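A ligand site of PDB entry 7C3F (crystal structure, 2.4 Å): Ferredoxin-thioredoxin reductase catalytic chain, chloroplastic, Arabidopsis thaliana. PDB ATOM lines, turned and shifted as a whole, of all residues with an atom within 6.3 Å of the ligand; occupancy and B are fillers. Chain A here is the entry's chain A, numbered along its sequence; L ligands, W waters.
The backbone NH (N) of Cys 75 lies close to a sulfur (S4) of the ligand, at 3.8 Å.
The side-chain sulfur (SG) of Cys 75 binds an iron atom (FE2) of the ligand (2.6 Å).
The side-chain sulfur (SG) of Cys 84 binds an iron atom (FE4) of the ligand, at 2.6 Å.
An iron atom (FE3) of the ligand is bound by the side-chain sulfur (SG) of Cys 73.
An iron atom (FE1) of the ligand is bound by the side-chain sulfur (SG) of Cys 54 (2.7 Å).
SG of Cys 86 lies close to S3 of the ligand (3.5 Å).
N of His 85 lies close to S3 of the ligand.
ND1 of His 85 sits close to S3 of the ligand (3.5 Å).
The side-chain sulfur of Cys 75 lies close to the backbone NH of Met 78 (3.3 Å).
The backbone NH (N) of Leu 88 lies close to the side-chain sulfur (SG) of Cys 84.
The side-chain sulfur (SG) of Cys 84 sits close to the backbone NH (N) of Met 87 (3.6 Å).
O of Pro 52 is in hydrogen-bond range of N of Cys 73, at 2.9 Å.
SG of Cys 54 lies close to SG of Cys 86, at 3.2 Å.
The backbone NH (N) of Cys 54 is in hydrogen-bond range of the backbone carbonyl oxygen (O) of Trp 71 (3.0 Å).
The side-chain sulfur (SG) of Cys 54 sits close to the backbone NH (N) of Cys 56, at 3.6 Å.
The side-chain sulfur (SG) of Cys 86 lies close to the side-chain sulfur (SG) of Cys 56, 3.8 Å away.
Merely in contact with the ligand: Met 78 (3.4 Å), Leu 88 (3.8 Å), Val 38 (3.9 Å) and Phe 89 (3.96 Å).
Hydrophobic or aromatic side chains within 4 Å of the ligand: Val 38, Met 78, His 85, Leu 88 and Phe 89.
Within 4 Å of the ligand: Val 38, Cys 54, Cys 73, Cys 75, Met 78, Cys 84, His 85, Cys 86, Leu 88 and Phe 89.
Along chain A the residues within 4 Å of the ligand span positions 38 to 89.
The nearest printed residue that does not touch the ligand is Pro 74 (4.04 Å).
Water W1 lies within hydrogen-bond range of ND1 of His 85 (2.9 Å), O of Glu 83 (3.1 Å) and S3 of the ligand (3.1 Å).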
ATOM      1  N   PHE A  16      -3.328 -14.262   0.309  1.00  0.00           N
ATOM      2  CA  PHE A  16      -3.316 -13.050  -0.495  1.00  0.00           C
ATOM      3  C   PHE A  16      -3.068 -13.364  -1.968  1.00  0.00           C
ATOM      4  O   PHE A  16      -3.701 -12.779  -2.853  1.00  0.00           O
ATOM      5  CB  PHE A  16      -2.248 -12.083   0.021  1.00  0.00           C
ATOM      6  CG  PHE A  16      -1.694 -11.181  -1.047  1.00  0.00           C
ATOM      7  CD1 PHE A  16      -2.380 -10.040  -1.437  1.00  0.00           C
ATOM      8  CD2 PHE A  16      -0.488 -11.473  -1.672  1.00  0.00           C
ATOM      9  CE1 PHE A  16      -1.883  -9.212  -2.419  1.00  0.00           C
ATOM     10  CE2 PHE A  16       0.017 -10.634  -2.661  1.00  0.00           C
ATOM     11  CZ  PHE A  16      -0.684  -9.500  -3.034  1.00  0.00           C
ATOM     12  N   TYR A  20      -5.271 -12.314  -4.880  1.00  0.00           N
ATOM     13  CA  TYR A  20      -4.801 -11.335  -5.860  1.00  0.00           C
ATOM     14  C   TYR A  20      -4.801 -11.907  -7.270  1.00  0.00           C
ATOM     15  O   TYR A  20      -4.909 -11.153  -8.231  1.00  0.00           O
ATOM     16  CB  TYR A  20      -3.408 -10.819  -5.474  1.00  0.00           C
ATOM     17  CG  TYR A  20      -3.054  -9.535  -6.192  1.00  0.00           C
ATOM     18  CD1 TYR A  20      -3.472  -8.306  -5.686  1.00  0.00           C
ATOM     19  CD2 TYR A  20      -2.329  -9.541  -7.378  1.00  0.00           C
ATOM     20  CE1 TYR A  20      -3.180  -7.121  -6.350  1.00  0.00           C
ATOM     21  CE2 TYR A  20      -2.030  -8.362  -8.044  1.00  0.00           C
ATOM     22  CZ  TYR A  20      -2.456  -7.164  -7.519  1.00  0.00           C
ATOM     23  OH  TYR A  20      -2.165  -5.996  -8.178  1.00  0.00           O
ATOM     24  N   VAL A  38       8.437 -18.160  -3.879  1.00  0.00           N
ATOM     25  CA  VAL A  38       8.225 -16.713  -3.843  1.00  0.00           C
ATOM     26  C   VAL A  38       7.313 -16.331  -2.675  1.00  0.00           C
ATOM     27  O   VAL A  38       7.579 -15.360  -1.960  1.00  0.00           O
ATOM     28  CB  VAL A  38       7.647 -16.213  -5.188  1.00  0.00           C
ATOM     29  CG1 VAL A  38       7.080 -14.807  -5.045  1.00  0.00           C
ATOM     30  CG2 VAL A  38       8.713 -16.257  -6.277  1.00  0.00           C
ATOM     31  N   LEU A  42       8.149 -13.744   0.304  1.00  0.00           N
ATOM     32  CA  LEU A  42       7.314 -12.655   0.776  1.00  0.00           C
ATOM     33  C   LEU A  42       7.040 -12.782   2.268  1.00  0.00           C
ATOM     34  O   LEU A  42       7.093 -11.794   3.005  1.00  0.00           O
ATOM     35  CB  LEU A  42       6.004 -12.608  -0.016  1.00  0.00           C
ATOM     36  CG  LEU A  42       6.151 -12.290  -1.496  1.00  0.00           C
ATOM     37  CD1 LEU A  42       4.872 -12.624  -2.264  1.00  0.00           C
ATOM     38  CD2 LEU A  42       6.530 -10.828  -1.679  1.00  0.00           C
ATOM     39  N   PRO A  52       5.669  -7.303   2.886  1.00  0.00           N
ATOM     40  CA  PRO A  52       6.180  -8.355   1.994  1.00  0.00           C
ATOM     41  C   PRO A  52       6.979  -7.762   0.834  1.00  0.00           C
ATOM     42  O   PRO A  52       6.532  -7.664  -0.314  1.00  0.00           O
ATOM     43  CB  PRO A  52       4.904  -9.066   1.530  1.00  0.00           C
ATOM     44  CG  PRO A  52       3.843  -8.023   1.601  1.00  0.00           C
ATOM     45  CD  PRO A  52       4.232  -7.035   2.687  1.00  0.00           C
ATOM     46  N   LEU A  53       8.206  -7.359   1.151  1.00  0.00           N
ATOM     47  CA  LEU A  53       9.135  -6.856   0.149  1.00  0.00           C
ATOM     48  C   LEU A  53       9.381  -7.935  -0.903  1.00  0.00           C
ATOM     49  O   LEU A  53       9.365  -9.129  -0.609  1.00  0.00           O
ATOM     50  CB  LEU A  53      10.459  -6.452   0.797  1.00  0.00           C
ATOM     51  CG  LEU A  53      10.834  -4.982   0.963  1.00  0.00           C
ATOM     52  CD1 LEU A  53      12.293  -4.870   1.377  1.00  0.00           C
ATOM     53  CD2 LEU A  53      10.565  -4.186  -0.307  1.00  0.00           C
ATOM     54  N   CYS A  54       9.617  -7.493  -2.133  1.00  0.00           N
ATOM     55  CA  CYS A  54       9.796  -8.437  -3.224  1.00  0.00           C
ATOM     56  C   CYS A  54      11.026  -9.293  -2.971  1.00  0.00           C
ATOM     57  O   CYS A  54      12.100  -8.752  -2.665  1.00  0.00           O
ATOM     58  CB  CYS A  54       9.949  -7.708  -4.552  1.00  0.00           C
ATOM     59  SG  CYS A  54      10.135  -8.808  -5.940  1.00  0.00           S
ATOM     60  N   PRO A  55      10.920 -10.615  -3.111  1.00  0.00           N
ATOM     61  CA  PRO A  55      12.055 -11.508  -2.826  1.00  0.00           C
ATOM     62  C   PRO A  55      12.991 -11.738  -4.009  1.00  0.00           C
ATOM     63  O   PRO A  55      13.981 -12.476  -3.857  1.00  0.00           O
ATOM     64  CB  PRO A  55      11.363 -12.819  -2.426  1.00  0.00           C
ATOM     65  CG  PRO A  55      10.065 -12.795  -3.195  1.00  0.00           C
ATOM     66  CD  PRO A  55       9.671 -11.347  -3.366  1.00  0.00           C
ATOM     67  N   CYS A  56      12.712 -11.153  -5.168  1.00  0.00           N
ATOM     68  CA  CYS A  56      13.590 -11.274  -6.323  1.00  0.00           C
ATOM     69  C   CYS A  56      14.216  -9.941  -6.688  1.00  0.00           C
ATOM     70  O   CYS A  56      14.524  -9.682  -7.855  1.00  0.00           O
ATOM     71  CB  CYS A  56      12.837 -11.870  -7.520  1.00  0.00           C
ATOM     72  SG  CYS A  56      12.515 -13.647  -7.382  1.00  0.00           S
ATOM     73  N   TRP A  71       8.336  -1.563  -3.765  1.00  0.00           N
ATOM     74  CA  TRP A  71       8.550  -3.000  -3.927  1.00  0.00           C
ATOM     75  C   TRP A  71       7.821  -3.829  -2.876  1.00  0.00           C
ATOM     76  O   TRP A  71       8.128  -5.016  -2.738  1.00  0.00           O
ATOM     77  CB  TRP A  71      10.043  -3.315  -3.915  1.00  0.00           C
ATOM     78  CG  TRP A  71      10.722  -2.947  -5.205  1.00  0.00           C
ATOM     79  CD1 TRP A  71      11.678  -1.992  -5.380  1.00  0.00           C
ATOM     80  CD2 TRP A  71      10.479  -3.518  -6.493  1.00  0.00           C
ATOM     81  NE1 TRP A  71      12.052  -1.931  -6.696  1.00  0.00           N
ATOM     82  CE2 TRP A  71      11.338  -2.860  -7.407  1.00  0.00           C
ATOM     83  CE3 TRP A  71       9.635  -4.524  -6.975  1.00  0.00           C
ATOM     84  CZ2 TRP A  71      11.358  -3.170  -8.767  1.00  0.00           C
ATOM     85  CZ3 TRP A  71       9.668  -4.838  -8.324  1.00  0.00           C
ATOM     86  CH2 TRP A  71      10.517  -4.158  -9.199  1.00  0.00           C
ATOM     87  N   ASN A  72       6.892  -3.243  -2.135  1.00  0.00           N
ATOM     88  CA  ASN A  72       6.028  -4.026  -1.270  1.00  0.00           C
ATOM     89  C   ASN A  72       4.973  -4.721  -2.131  1.00  0.00           C
ATOM     90  O   ASN A  72       4.284  -4.063  -2.916  1.00  0.00           O
ATOM     91  CB  ASN A  72       5.361  -3.148  -0.211  1.00  0.00           C
ATOM     92  CG  ASN A  72       6.353  -2.622   0.826  1.00  0.00           C
ATOM     93  OD1 ASN A  72       7.482  -3.093   0.943  1.00  0.00           O
ATOM     94  ND2 ASN A  72       5.920  -1.630   1.604  1.00  0.00           N
ATOM     95  N   CYS A  73       4.852  -6.030  -1.976  1.00  0.00           N
ATOM     96  CA  CYS A  73       3.997  -6.802  -2.863  1.00  0.00           C
ATOM     97  C   CYS A  73       2.524  -6.514  -2.572  1.00  0.00           C
ATOM     98  O   CYS A  73       2.112  -6.509  -1.405  1.00  0.00           O
ATOM     99  CB  CYS A  73       4.290  -8.291  -2.672  1.00  0.00           C
ATOM    100  SG  CYS A  73       3.306  -9.482  -3.583  1.00  0.00           S
ATOM    101  N   PRO A  74       1.687  -6.287  -3.602  1.00  0.00           N
ATOM    102  CA  PRO A  74       2.062  -6.193  -5.023  1.00  0.00           C
ATOM    103  C   PRO A  74       2.828  -4.921  -5.380  1.00  0.00           C
ATOM    104  O   PRO A  74       2.311  -3.828  -5.172  1.00  0.00           O
ATOM    105  CB  PRO A  74       0.710  -6.232  -5.735  1.00  0.00           C
ATOM    106  CG  PRO A  74      -0.268  -5.735  -4.730  1.00  0.00           C
ATOM    107  CD  PRO A  74       0.233  -6.177  -3.401  1.00  0.00           C
ATOM    108  N   CYS A  75       4.055  -5.090  -5.891  1.00  0.00           N
ATOM    109  CA  CYS A  75       4.858  -3.980  -6.373  1.00  0.00           C
ATOM    110  C   CYS A  75       4.086  -3.095  -7.355  1.00  0.00           C
ATOM    111  O   CYS A  75       3.169  -3.556  -8.049  1.00  0.00           O
ATOM    112  CB  CYS A  75       6.129  -4.507  -7.033  1.00  0.00           C
ATOM    113  SG  CYS A  75       5.911  -5.260  -8.671  1.00  0.00           S
ATOM    114  N   VAL A  76       4.438  -1.818  -7.375  1.00  0.00           N
ATOM    115  CA  VAL A  76       4.009  -0.841  -8.381  1.00  0.00           C
ATOM    116  C   VAL A  76       3.966  -1.429  -9.790  1.00  0.00           C
ATOM    117  O   VAL A  76       2.925  -1.277 -10.467  1.00  0.00           O
ATOM    118  CB  VAL A  76       4.893   0.413  -8.315  1.00  0.00           C
ATOM    119  CG1 VAL A  76       4.796   1.205  -9.605  1.00  0.00           C
ATOM    120  CG2 VAL A  76       4.514   1.274  -7.122  1.00  0.00           C
ATOM    121  N   PRO A  77       5.027  -2.064 -10.303  1.00  0.00           N
ATOM    122  CA  PRO A  77       4.925  -2.626 -11.664  1.00  0.00           C
ATOM    123  C   PRO A  77       3.816  -3.655 -11.831  1.00  0.00           C
ATOM    124  O   PRO A  77       3.214  -3.745 -12.914  1.00  0.00           O
ATOM    125  CB  PRO A  77       6.304  -3.263 -11.884  1.00  0.00           C
ATOM    126  CG  PRO A  77       7.206  -2.443 -11.040  1.00  0.00           C
ATOM    127  CD  PRO A  77       6.415  -2.131  -9.803  1.00  0.00           C
ATOM    128  N   MET A  78       3.506  -4.434 -10.792  1.00  0.00           N
ATOM    129  CA  MET A  78       2.415  -5.388 -10.896  1.00  0.00           C
ATOM    130  C   MET A  78       1.073  -4.701 -10.804  1.00  0.00           C
ATOM    131  O   MET A  78       0.133  -5.037 -11.547  1.00  0.00           O
ATOM    132  CB  MET A  78       2.538  -6.454  -9.798  1.00  0.00           C
ATOM    133  CG  MET A  78       1.381  -7.430  -9.775  1.00  0.00           C
ATOM    134  SD  MET A  78       1.306  -8.431 -11.274  1.00  0.00           S
ATOM    135  CE  MET A  78      -0.398  -9.002 -11.208  1.00  0.00           C
ATOM    136  N   ARG A  79       0.936  -3.731  -9.894  1.00  0.00           N
ATOM    137  CA  ARG A  79      -0.325  -3.019  -9.743  1.00  0.00           C
ATOM    138  C   ARG A  79      -0.659  -2.210 -10.991  1.00  0.00           C
ATOM    139  O   ARG A  79      -1.819  -2.147 -11.410  1.00  0.00           O
ATOM    140  CB  ARG A  79      -0.273  -2.108  -8.518  1.00  0.00           C
ATOM    141  CG  ARG A  79      -0.383  -2.847  -7.201  1.00  0.00           C
ATOM    142  CD  ARG A  79      -0.832  -1.912  -6.103  1.00  0.00           C
ATOM    143  NE  ARG A  79       0.263  -1.055  -5.671  1.00  0.00           N
ATOM    144  CZ  ARG A  79       0.674  -0.971  -4.410  1.00  0.00           C
ATOM    145  NH1 ARG A  79       1.677  -0.167  -4.082  1.00  0.00           N
ATOM    146  NH2 ARG A  79       0.075  -1.701  -3.472  1.00  0.00           N
ATOM    147  N   GLU A  83       2.952  -6.592 -14.367  1.00  0.00           N
ATOM    148  CA  GLU A  83       4.266  -7.199 -14.569  1.00  0.00           C
ATOM    149  C   GLU A  83       4.788  -7.711 -13.234  1.00  0.00           C
ATOM    150  O   GLU A  83       5.009  -6.934 -12.297  1.00  0.00           O
ATOM    151  CB  GLU A  83       5.240  -6.182 -15.172  1.00  0.00           C
ATOM    152  CG  GLU A  83       4.931  -5.840 -16.623  1.00  0.00           C
ATOM    153  CD  GLU A  83       5.816  -4.715 -17.158  1.00  0.00           C
ATOM    154  OE1 GLU A  83       5.526  -4.219 -18.267  1.00  0.00           O
ATOM    155  OE2 GLU A  83       6.782  -4.338 -16.461  1.00  0.00           O
ATOM    156  N   CYS A  84       4.977  -9.026 -13.144  1.00  0.00           N
ATOM    157  CA  CYS A  84       5.500  -9.677 -11.938  1.00  0.00           C
ATOM    158  C   CYS A  84       6.721 -10.490 -12.337  1.00  0.00           C
ATOM    159  O   CYS A  84       6.595 -11.553 -12.948  1.00  0.00           O
ATOM    160  CB  CYS A  84       4.417 -10.542 -11.284  1.00  0.00           C
ATOM    161  SG  CYS A  84       5.005 -11.821 -10.159  1.00  0.00           S
ATOM    162  N   HIS A  85       7.920  -9.992 -11.995  1.00  0.00           N
ATOM    163  CA  HIS A  85       9.159 -10.623 -12.429  1.00  0.00           C
ATOM    164  C   HIS A  85       9.608 -11.761 -11.517  1.00  0.00           C
ATOM    165  O   HIS A  85      10.591 -12.436 -11.837  1.00  0.00           O
ATOM    166  CB  HIS A  85      10.282  -9.581 -12.547  1.00  0.00           C
ATOM    167  CG  HIS A  85      10.855  -9.156 -11.236  1.00  0.00           C
ATOM    168  ND1 HIS A  85      10.279  -8.190 -10.437  1.00  0.00           N
ATOM    169  CD2 HIS A  85      11.966  -9.575 -10.573  1.00  0.00           C
ATOM    170  CE1 HIS A  85      11.009  -8.025  -9.347  1.00  0.00           C
ATOM    171  NE2 HIS A  85      12.034  -8.855  -9.401  1.00  0.00           N
ATOM    172  N   CYS A  86       8.901 -12.013 -10.410  1.00  0.00           N
ATOM    173  CA  CYS A  86       9.120 -13.244  -9.660  1.00  0.00           C
ATOM    174  C   CYS A  86       8.300 -14.385 -10.204  1.00  0.00           C
ATOM    175  O   CYS A  86       8.372 -15.498  -9.667  1.00  0.00           O
ATOM    176  CB  CYS A  86       8.785 -13.073  -8.175  1.00  0.00           C
ATOM    177  SG  CYS A  86       9.361 -11.553  -7.468  1.00  0.00           S
ATOM    178  N   MET A  87       7.529 -14.137 -11.265  1.00  0.00           N
ATOM    179  CA  MET A  87       6.689 -15.152 -11.901  1.00  0.00           C
ATOM    180  C   MET A  87       5.737 -15.776 -10.883  1.00  0.00           C
ATOM    181  O   MET A  87       5.454 -16.973 -10.924  1.00  0.00           O
ATOM    182  CB  MET A  87       7.561 -16.210 -12.584  1.00  0.00           C
ATOM    183  CG  MET A  87       8.605 -15.589 -13.510  1.00  0.00           C
ATOM    184  SD  MET A  87       9.586 -16.770 -14.438  1.00  0.00           S
ATOM    185  CE  MET A  87       8.295 -17.807 -15.118  1.00  0.00           C
ATOM    186  N   LEU A  88       5.244 -14.938  -9.966  1.00  0.00           N
ATOM    187  CA  LEU A  88       4.167 -15.343  -9.067  1.00  0.00           C
ATOM    188  C   LEU A  88       2.807 -15.150  -9.730  1.00  0.00           C
ATOM    189  O   LEU A  88       1.985 -16.069  -9.735  1.00  0.00           O
ATOM    190  CB  LEU A  88       4.254 -14.555  -7.758  1.00  0.00           C
ATOM    191  CG  LEU A  88       3.103 -14.680  -6.765  1.00  0.00           C
ATOM    192  CD1 LEU A  88       2.838 -16.136  -6.399  1.00  0.00           C
ATOM    193  CD2 LEU A  88       3.392 -13.868  -5.507  1.00  0.00           C
ATOM    194  N   PHE A  89       2.559 -13.965 -10.285  1.00  0.00           N
ATOM    195  CA  PHE A  89       1.323 -13.654 -10.990  1.00  0.00           C
ATOM    196  C   PHE A  89       1.659 -13.495 -12.464  1.00  0.00           C
ATOM    197  O   PHE A  89       2.368 -12.561 -12.850  1.00  0.00           O
ATOM    198  CB  PHE A  89       0.662 -12.382 -10.454  1.00  0.00           C
ATOM    199  CG  PHE A  89       0.510 -12.346  -8.964  1.00  0.00           C
ATOM    200  CD1 PHE A  89      -0.415 -13.167  -8.335  1.00  0.00           C
ATOM    201  CD2 PHE A  89       1.282 -11.493  -8.192  1.00  0.00           C
ATOM    202  CE1 PHE A  89      -0.559 -13.134  -6.954  1.00  0.00           C
ATOM    203  CE2 PHE A  89       1.139 -11.460  -6.811  1.00  0.00           C
ATOM    204  CZ  PHE A  89       0.208 -12.284  -6.194  1.00  0.00           C
HETATM  205 FE1  LIG L   1       7.573  -9.524  -6.462  1.00  0.00          FE
HETATM  206 FE2  LIG L   1       5.967  -7.547  -7.465  1.00  0.00          FE
HETATM  207 FE3  LIG L   1       4.942  -9.334  -5.673  1.00  0.00          FE
HETATM  208 FE4  LIG L   1       5.568 -10.164  -8.192  1.00  0.00          FE
HETATM  209  S1  LIG L   1       3.970  -8.642  -7.608  1.00  0.00           S
HETATM  210  S2  LIG L   1       6.070 -11.231  -6.257  1.00  0.00           S
HETATM  211  S3  LIG L   1       7.412  -8.884  -8.646  1.00  0.00           S
HETATM  212  S4  LIG L   1       6.600  -7.805  -5.299  1.00  0.00           S
HETATM  213  O   HOH W   1       7.783  -6.858 -10.966  1.00  0.00           O
